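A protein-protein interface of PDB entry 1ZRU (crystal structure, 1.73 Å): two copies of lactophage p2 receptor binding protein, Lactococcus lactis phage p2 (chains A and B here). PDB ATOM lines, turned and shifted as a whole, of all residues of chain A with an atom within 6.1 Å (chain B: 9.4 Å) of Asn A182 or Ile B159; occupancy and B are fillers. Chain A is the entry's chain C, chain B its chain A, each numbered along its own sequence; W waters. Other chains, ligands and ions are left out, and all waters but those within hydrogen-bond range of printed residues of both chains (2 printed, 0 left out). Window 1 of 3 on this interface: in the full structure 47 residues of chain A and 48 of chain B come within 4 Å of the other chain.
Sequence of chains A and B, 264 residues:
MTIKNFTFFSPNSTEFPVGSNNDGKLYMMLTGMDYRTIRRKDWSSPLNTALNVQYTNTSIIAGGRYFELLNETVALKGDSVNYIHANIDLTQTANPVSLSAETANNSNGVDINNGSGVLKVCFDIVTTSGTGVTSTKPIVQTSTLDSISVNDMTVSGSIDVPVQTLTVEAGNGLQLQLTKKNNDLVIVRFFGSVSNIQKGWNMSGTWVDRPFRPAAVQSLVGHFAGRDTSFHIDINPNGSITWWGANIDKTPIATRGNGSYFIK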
ATOM      1  N   ILE A 159     -18.874 -21.838 -19.174  1.00  0.00           N
ATOM      2  CA  ILE A 159     -17.917 -21.044 -18.417  1.00  0.00           C
ATOM      3  C   ILE A 159     -17.038 -20.276 -19.395  1.00  0.00           C
ATOM      4  O   ILE A 159     -16.419 -20.874 -20.298  1.00  0.00           O
ATOM      5  CB  ILE A 159     -17.019 -21.904 -17.523  1.00  0.00           C
ATOM      6  CG1 ILE A 159     -17.857 -22.793 -16.598  1.00  0.00           C
ATOM      7  CG2 ILE A 159     -16.013 -21.015 -16.731  1.00  0.00           C
ATOM      8  CD1 ILE A 159     -17.033 -23.789 -15.757  1.00  0.00           C
ATOM      9  N   VAL A 161     -13.641 -18.356 -19.625  1.00  0.00           N
ATOM     10  CA  VAL A 161     -12.361 -18.120 -18.927  1.00  0.00           C
ATOM     11  C   VAL A 161     -11.427 -17.266 -19.803  1.00  0.00           C
ATOM     12  O   VAL A 161     -11.664 -17.156 -21.005  1.00  0.00           O
ATOM     13  CB  VAL A 161     -11.631 -19.444 -18.525  1.00  0.00           C
ATOM     14  CG1 VAL A 161     -12.477 -20.282 -17.566  1.00  0.00           C
ATOM     15  CG2 VAL A 161     -11.236 -20.262 -19.770  1.00  0.00           C
ATOM     16  N   PRO A 162     -10.401 -16.639 -19.200  1.00  0.00           N
ATOM     17  CA  PRO A 162      -9.522 -15.796 -20.022  1.00  0.00           C
ATOM     18  C   PRO A 162      -8.790 -16.586 -21.101  1.00  0.00           C
ATOM     19  O   PRO A 162      -8.452 -17.760 -20.906  1.00  0.00           O
ATOM     20  CB  PRO A 162      -8.517 -15.252 -19.014  1.00  0.00           C
ATOM     21  CG  PRO A 162      -9.299 -15.234 -17.692  1.00  0.00           C
ATOM     22  CD  PRO A 162     -10.035 -16.559 -17.767  1.00  0.00           C
ATOM     23  N   VAL A 163      -8.569 -15.920 -22.226  1.00  0.00           N
ATOM     24  CA  VAL A 163      -7.876 -16.516 -23.360  1.00  0.00           C
ATOM     25  C   VAL A 163      -6.789 -15.553 -23.824  1.00  0.00           C
ATOM     26  O   VAL A 163      -7.020 -14.336 -23.924  1.00  0.00           O
ATOM     27  CB  VAL A 163      -8.846 -16.786 -24.535  1.00  0.00           C
ATOM     28  CG1 VAL A 163      -8.097 -17.399 -25.732  1.00  0.00           C
ATOM     29  CG2 VAL A 163     -10.010 -17.680 -24.113  1.00  0.00           C
ATOM     30  N   LYS A 180      -3.961 -20.022 -25.221  1.00  0.00           N
ATOM     31  CA  LYS A 180      -3.913 -20.464 -23.836  1.00  0.00           C
ATOM     32  C   LYS A 180      -5.219 -20.073 -23.150  1.00  0.00           C
ATOM     33  O   LYS A 180      -5.667 -18.926 -23.281  1.00  0.00           O
ATOM     34  CB  LYS A 180      -2.732 -19.780 -23.151  1.00  0.00           C
ATOM     35  CG  LYS A 180      -2.577 -20.090 -21.680  1.00  0.00           C
ATOM     36  CD  LYS A 180      -1.398 -19.289 -21.074  1.00  0.00           C
ATOM     37  CE  LYS A 180      -1.641 -17.785 -21.175  1.00  0.00           C
ATOM     38  NZ  LYS A 180      -1.051 -17.045 -20.051  1.00  0.00           N
ATOM     39  N   LYS A 181      -5.837 -21.030 -22.465  1.00  0.00           N
ATOM     40  CA  LYS A 181      -7.084 -20.750 -21.745  1.00  0.00           C
ATOM     41  C   LYS A 181      -6.920 -21.026 -20.253  1.00  0.00           C
ATOM     42  O   LYS A 181      -6.229 -21.958 -19.848  1.00  0.00           O
ATOM     43  CB  LYS A 181      -8.269 -21.517 -22.347  1.00  0.00           C
ATOM     44  CG  LYS A 181      -8.480 -21.194 -23.831  1.00  0.00           C
ATOM     45  CD  LYS A 181      -9.886 -21.446 -24.337  1.00  0.00           C
ATOM     46  CE  LYS A 181      -9.944 -21.125 -25.832  1.00  0.00           C
ATOM     47  NZ  LYS A 181     -11.373 -21.128 -26.356  1.00  0.00           N
ATOM     48  N   ASN A 182      -7.558 -20.194 -19.428  1.00  0.00           N
ATOM     49  CA  ASN A 182      -7.460 -20.329 -17.967  1.00  0.00           C
ATOM     50  C   ASN A 182      -6.007 -20.287 -17.466  1.00  0.00           C
ATOM     51  O   ASN A 182      -5.643 -20.913 -16.461  1.00  0.00           O
ATOM     52  CB  ASN A 182      -8.189 -21.601 -17.491  1.00  0.00           C
ATOM     53  CG  ASN A 182      -8.429 -21.602 -15.992  1.00  0.00           C
ATOM     54  OD1 ASN A 182      -8.791 -20.571 -15.415  1.00  0.00           O
ATOM     55  ND2 ASN A 182      -8.190 -22.742 -15.350  1.00  0.00           N
ATOM     56  N   ASN A 183      -5.170 -19.553 -18.202  1.00  0.00           N
ATOM     57  CA  ASN A 183      -3.743 -19.461 -17.936  1.00  0.00           C
ATOM     58  C   ASN A 183      -3.086 -20.833 -17.713  1.00  0.00           C
ATOM     59  O   ASN A 183      -2.158 -20.978 -16.915  1.00  0.00           O
ATOM     60  CB  ASN A 183      -3.475 -18.526 -16.741  1.00  0.00           C
ATOM     61  CG  ASN A 183      -2.022 -18.088 -16.657  1.00  0.00           C
ATOM     62  OD1 ASN A 183      -1.305 -18.007 -17.668  1.00  0.00           O
ATOM     63  ND2 ASN A 183      -1.566 -17.818 -15.430  1.00  0.00           N
ATOM     64  N   ASP A 184      -3.554 -21.845 -18.436  1.00  0.00           N
ATOM     65  CA  ASP A 184      -3.075 -23.194 -18.177  1.00  0.00           C
ATOM     66  C   ASP A 184      -3.041 -24.124 -19.383  1.00  0.00           C
ATOM     67  O   ASP A 184      -1.978 -24.636 -19.726  1.00  0.00           O
ATOM     68  CB  ASP A 184      -3.835 -23.853 -17.029  1.00  0.00           C
ATOM     69  CG  ASP A 184      -3.205 -25.163 -16.613  1.00  0.00           C
ATOM     70  OD1 ASP A 184      -1.950 -25.220 -16.492  1.00  0.00           O
ATOM     71  OD2 ASP A 184      -3.957 -26.121 -16.413  1.00  0.00           O
ATOM     72  N   LEU A 185      -4.178 -24.329 -20.035  1.00  0.00           N
ATOM     73  CA  LEU A 185      -4.220 -25.258 -21.157  1.00  0.00           C
ATOM     74  C   LEU A 185      -3.849 -24.519 -22.434  1.00  0.00           C
ATOM     75  O   LEU A 185      -4.471 -23.520 -22.760  1.00  0.00           O
ATOM     76  CB  LEU A 185      -5.621 -25.857 -21.300  1.00  0.00           C
ATOM     77  CG  LEU A 185      -5.825 -26.770 -22.519  1.00  0.00           C
ATOM     78  CD1 LEU A 185      -4.845 -27.963 -22.524  1.00  0.00           C
ATOM     79  CD2 LEU A 185      -7.278 -27.235 -22.614  1.00  0.00           C
ATOM     80  N   LYS A 264       1.025 -25.494 -16.061  1.00  0.00           N
ATOM     81  CA  LYS A 264       1.236 -25.823 -14.655  1.00  0.00           C
ATOM     82  C   LYS A 264       1.209 -27.337 -14.418  1.00  0.00           C
ATOM     83  O   LYS A 264       0.251 -28.030 -14.820  1.00  0.00           O
ATOM     84  CB  LYS A 264       0.157 -25.151 -13.801  1.00  0.00           C
ATOM     85  CG  LYS A 264       0.028 -23.647 -13.991  1.00  0.00           C
ATOM     86  CD  LYS A 264      -1.217 -23.125 -13.282  1.00  0.00           C
ATOM     87  CE  LYS A 264      -1.607 -21.763 -13.809  1.00  0.00           C
ATOM     88  NZ  LYS A 264      -2.589 -21.093 -12.909  1.00  0.00           N
ATOM     89  N   MET B 153     -21.043 -18.710 -16.212  1.00  0.00           N
ATOM     90  CA  MET B 153     -20.056 -18.100 -15.345  1.00  0.00           C
ATOM     91  C   MET B 153     -18.992 -17.431 -16.185  1.00  0.00           C
ATOM     92  O   MET B 153     -18.592 -17.975 -17.208  1.00  0.00           O
ATOM     93  CB  MET B 153     -19.397 -19.141 -14.443  1.00  0.00           C
ATOM     94  CG  MET B 153     -18.304 -18.532 -13.556  1.00  0.00           C
ATOM     95  SD  MET B 153     -17.691 -19.687 -12.299  1.00  0.00           S
ATOM     96  CE  MET B 153     -16.983 -20.983 -13.269  1.00  0.00           C
ATOM     97  N   THR B 154     -18.575 -16.238 -15.773  1.00  0.00           N
ATOM     98  CA  THR B 154     -17.436 -15.571 -16.400  1.00  0.00           C
ATOM     99  C   THR B 154     -16.374 -15.391 -15.333  1.00  0.00           C
ATOM    100  O   THR B 154     -16.668 -14.886 -14.244  1.00  0.00           O
ATOM    101  CB  THR B 154     -17.829 -14.210 -16.980  1.00  0.00           C
ATOM    102  OG1 THR B 154     -18.876 -14.406 -17.945  1.00  0.00           O
ATOM    103  CG2 THR B 154     -16.624 -13.558 -17.658  1.00  0.00           C
ATOM    104  N   VAL B 155     -15.144 -15.815 -15.641  1.00  0.00           N
ATOM    105  CA  VAL B 155     -14.018 -15.764 -14.707  1.00  0.00           C
ATOM    106  C   VAL B 155     -12.972 -14.790 -15.251  1.00  0.00           C
ATOM    107  O   VAL B 155     -12.492 -14.976 -16.372  1.00  0.00           O
ATOM    108  CB  VAL B 155     -13.371 -17.180 -14.577  1.00  0.00           C
ATOM    109  CG1 VAL B 155     -12.076 -17.151 -13.716  1.00  0.00           C
ATOM    110  CG2 VAL B 155     -14.403 -18.200 -14.040  1.00  0.00           C
ATOM    111  N   SER B 156     -12.613 -13.768 -14.475  1.00  0.00           N
ATOM    112  CA  SER B 156     -11.600 -12.800 -14.954  1.00  0.00           C
ATOM    113  C   SER B 156     -10.171 -13.192 -14.578  1.00  0.00           C
ATOM    114  O   SER B 156      -9.209 -12.772 -15.251  1.00  0.00           O
ATOM    115  CB  SER B 156     -11.911 -11.389 -14.457  1.00  0.00           C
ATOM    116  OG  SER B 156     -11.964 -11.364 -13.049  1.00  0.00           O
ATOM    117  N   GLY B 157     -10.032 -13.975 -13.506  1.00  0.00           N
ATOM    118  CA  GLY B 157      -8.743 -14.461 -13.013  1.00  0.00           C
ATOM    119  C   GLY B 157      -8.529 -15.877 -13.517  1.00  0.00           C
ATOM    120  O   GLY B 157      -8.411 -16.084 -14.723  1.00  0.00           O
ATOM    121  N   SER B 158      -8.511 -16.854 -12.617  1.00  0.00           N
ATOM    122  CA  SER B 158      -8.322 -18.254 -13.019  1.00  0.00           C
ATOM    123  C   SER B 158      -9.192 -19.183 -12.185  1.00  0.00           C
ATOM    124  O   SER B 158      -9.578 -18.839 -11.069  1.00  0.00           O
ATOM    125  CB  SER B 158      -6.851 -18.675 -12.858  1.00  0.00           C
ATOM    126  OG  SER B 158      -6.013 -18.067 -13.845  1.00  0.00           O
ATOM    127  N   ILE B 159      -9.499 -20.351 -12.740  1.00  0.00           N
ATOM    128  CA  ILE B 159     -10.098 -21.425 -11.948  1.00  0.00           C
ATOM    129  C   ILE B 159      -9.020 -22.419 -11.588  1.00  0.00           C
ATOM    130  O   ILE B 159      -8.291 -22.906 -12.473  1.00  0.00           O
ATOM    131  CB  ILE B 159     -11.221 -22.162 -12.681  1.00  0.00           C
ATOM    132  CG1 ILE B 159     -12.294 -21.195 -13.177  1.00  0.00           C
ATOM    133  CG2 ILE B 159     -11.837 -23.244 -11.748  1.00  0.00           C
ATOM    134  CD1 ILE B 159     -13.322 -21.839 -14.080  1.00  0.00           C
ATOM    135  N   ASP B 160      -8.896 -22.705 -10.293  1.00  0.00           N
ATOM    136  CA  ASP B 160      -8.010 -23.760  -9.821  1.00  0.00           C
ATOM    137  C   ASP B 160      -8.807 -25.040  -9.612  1.00  0.00           C
ATOM    138  O   ASP B 160      -9.675 -25.096  -8.733  1.00  0.00           O
ATOM    139  CB  ASP B 160      -7.327 -23.365  -8.509  1.00  0.00           C
ATOM    140  CG  ASP B 160      -6.491 -24.503  -7.935  1.00  0.00           C
ATOM    141  OD1 ASP B 160      -6.863 -25.064  -6.882  1.00  0.00           O
ATOM    142  OD2 ASP B 160      -5.478 -24.867  -8.567  1.00  0.00           O
ATOM    143  N   VAL B 161      -8.531 -26.068 -10.414  1.00  0.00           N
ATOM    144  CA  VAL B 161      -9.190 -27.377 -10.237  1.00  0.00           C
ATOM    145  C   VAL B 161      -8.154 -28.411  -9.761  1.00  0.00           C
ATOM    146  O   VAL B 161      -6.948 -28.180  -9.917  1.00  0.00           O
ATOM    147  CB  VAL B 161      -9.874 -27.881 -11.551  1.00  0.00           C
ATOM    148  CG1 VAL B 161     -11.013 -26.932 -11.977  1.00  0.00           C
ATOM    149  CG2 VAL B 161      -8.832 -28.053 -12.681  1.00  0.00           C
ATOM    150  N   PRO B 162      -8.612 -29.534  -9.176  1.00  0.00           N
ATOM    151  CA  PRO B 162      -7.676 -30.563  -8.721  1.00  0.00           C
ATOM    152  C   PRO B 162      -6.806 -31.109  -9.841  1.00  0.00           C
ATOM    153  O   PRO B 162      -7.247 -31.207 -10.986  1.00  0.00           O
ATOM    154  CB  PRO B 162      -8.593 -31.659  -8.186  1.00  0.00           C
ATOM    155  CG  PRO B 162      -9.818 -30.883  -7.717  1.00  0.00           C
ATOM    156  CD  PRO B 162     -10.008 -29.900  -8.828  1.00  0.00           C
ATOM    157  N   VAL B 163      -5.576 -31.445  -9.479  1.00  0.00           N
ATOM    158  CA  VAL B 163      -4.617 -32.004 -10.435  1.00  0.00           C
ATOM    159  C   VAL B 163      -3.998 -33.241  -9.796  1.00  0.00           C
ATOM    160  O   VAL B 163      -3.600 -33.193  -8.624  1.00  0.00           O
ATOM    161  CB  VAL B 163      -3.507 -30.979 -10.776  1.00  0.00           C
ATOM    162  CG1 VAL B 163      -2.477 -31.584 -11.769  1.00  0.00           C
ATOM    163  CG2 VAL B 163      -4.097 -29.673 -11.331  1.00  0.00           C
ATOM    164  N   LYS B 181      -6.545 -33.297 -14.861  1.00  0.00           N
ATOM    165  CA  LYS B 181      -7.152 -32.098 -14.252  1.00  0.00           C
ATOM    166  C   LYS B 181      -8.678 -32.197 -14.234  1.00  0.00           C
ATOM    167  O   LYS B 181      -9.296 -32.724 -15.164  1.00  0.00           O
ATOM    168  CB  LYS B 181      -6.686 -30.832 -14.973  1.00  0.00           C
ATOM    169  CG  LYS B 181      -5.177 -30.667 -14.930  1.00  0.00           C
ATOM    170  CD  LYS B 181      -4.721 -29.248 -14.984  1.00  0.00           C
ATOM    171  CE  LYS B 181      -3.211 -29.225 -14.983  1.00  0.00           C
ATOM    172  NZ  LYS B 181      -2.614 -27.852 -14.892  1.00  0.00           N
ATOM    173  N   ASN B 182      -9.289 -31.694 -13.159  1.00  0.00           N
ATOM    174  CA  ASN B 182     -10.743 -31.792 -12.974  1.00  0.00           C
ATOM    175  C   ASN B 182     -11.268 -33.234 -13.065  1.00  0.00           C
ATOM    176  O   ASN B 182     -12.405 -33.474 -13.514  1.00  0.00           O
ATOM    177  CB  ASN B 182     -11.456 -30.878 -13.991  1.00  0.00           C
ATOM    178  CG  ASN B 182     -12.922 -30.610 -13.628  1.00  0.00           C
ATOM    179  OD1 ASN B 182     -13.246 -30.351 -12.477  1.00  0.00           O
ATOM    180  ND2 ASN B 182     -13.804 -30.706 -14.617  1.00  0.00           N
HETATM  181  O   HOH W   1      -6.882 -17.411 -16.418  1.00  0.00           O
HETATM  182  O   HOH W   2      -3.231 -18.557 -13.091  1.00  0.00           O
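N of Lys A264 lies within hydrogen-bond range of OD1 of Asp A184.
O of Pro A162 is in hydrogen-bond range of N of Asn A182, 3.0 Å away.
The side-chain amide oxygen (OD1) of Asn A183 sits at hydrogen-bond distance from the side-chain amino group (NZ) of Lys A180 (2.6 Å).
Ile A159 touches its own counterpart, Ile B159.
Val A161 touches Ile B159, but with the chains exchanged Ile A159 does not touch Val B161 (7.8 Å).
Asn A182 touches Ile B159, but with the chains exchanged Ile A159 does not touch Asn B182 (7.7 Å).
Among the printed residues, pairs that only touch across the chains: Pro A162 with Gly B157 (3.2 Å), Pro A162 with Val B155 (3.2 Å), Asn A182 with Ser B158 (3.4 Å), Ile A159 with Met B153 (3.4 Å), Pro A162 with Ser B156 (3.5 Å), Ile A159 with Ile B159 (3.9 Å), Asn A183 with Ser B158 (3.9 Å) and Val A161 with Ile B159 (3.9 Å).
Water W2 lies within hydrogen-bond range of NZ of Lys A264, OG of Ser B158 and ND2 of Asn A183.
Water W1 lies within hydrogen-bond range of O of Gly B157 (2.6 Å), OG of Ser B158 (2.8 Å) and N of Asn A183 (3.3 Å).
Asn A182 touches just these residues of chain B: Ser B158 and Ile B159.
Of the printed residues of chain B, Asn A183 touches Ser B158.
Thr B154 touches none of the printed residues of chain A.
Of the printed residues of chain A, Ser B156 touches Pro A162.
Of the printed residues of chain A, Ser B158 touches Asn A182 and Asn A183.
Of chain A, only Ile A159, Val A161 and Asn A182 come within 4 Å of Ile B159.
Asn B182 touches none of the printed residues of chain A.
The nearest residue of chain B that does not touch Asn A182 is Gly B157 (4.6 Å).
The nearest residue of chain A that does not touch Ile B159 is Lys A264 (6.0 Å).
The nearest printed residue of chain A that does not touch Ser B156 is Val A161 (6.2 Å).
Of the 13 printed residues of chain B, 7 touch a printed residue of chain A.
Along chain B the printed residues that touch a printed residue of chain A span positions 153 to 181.
Printed residues of chain A that touch a printed residue of chain B: Ile A159, Val A161, Pro A162, Asn A182, Asn A183, Asp A184 and Lys A264.
Among the printed residues, 11 pairs touch across the chains.
Among the printed residues, Asp or Glu carboxylates within 4 Å of a Lys or Arg side-chain nitrogen of the other chain: Asp A184 with Lys B181 (2.7 Å).
The side-chain amino group of Lys B181 lies within hydrogen-bond range of the backbone carbonyl oxygen of Lys A264, at 2.9 Å.
The side-chain amino group (NZ) of Lys B181 is in salt-bridge range of the side-chain carboxylate (OD2) of Asp A184, at 2.7 Å.
OD1 of Asn A182 sits at hydrogen-bond distance from N of Ile B159, 2.8 Å away.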
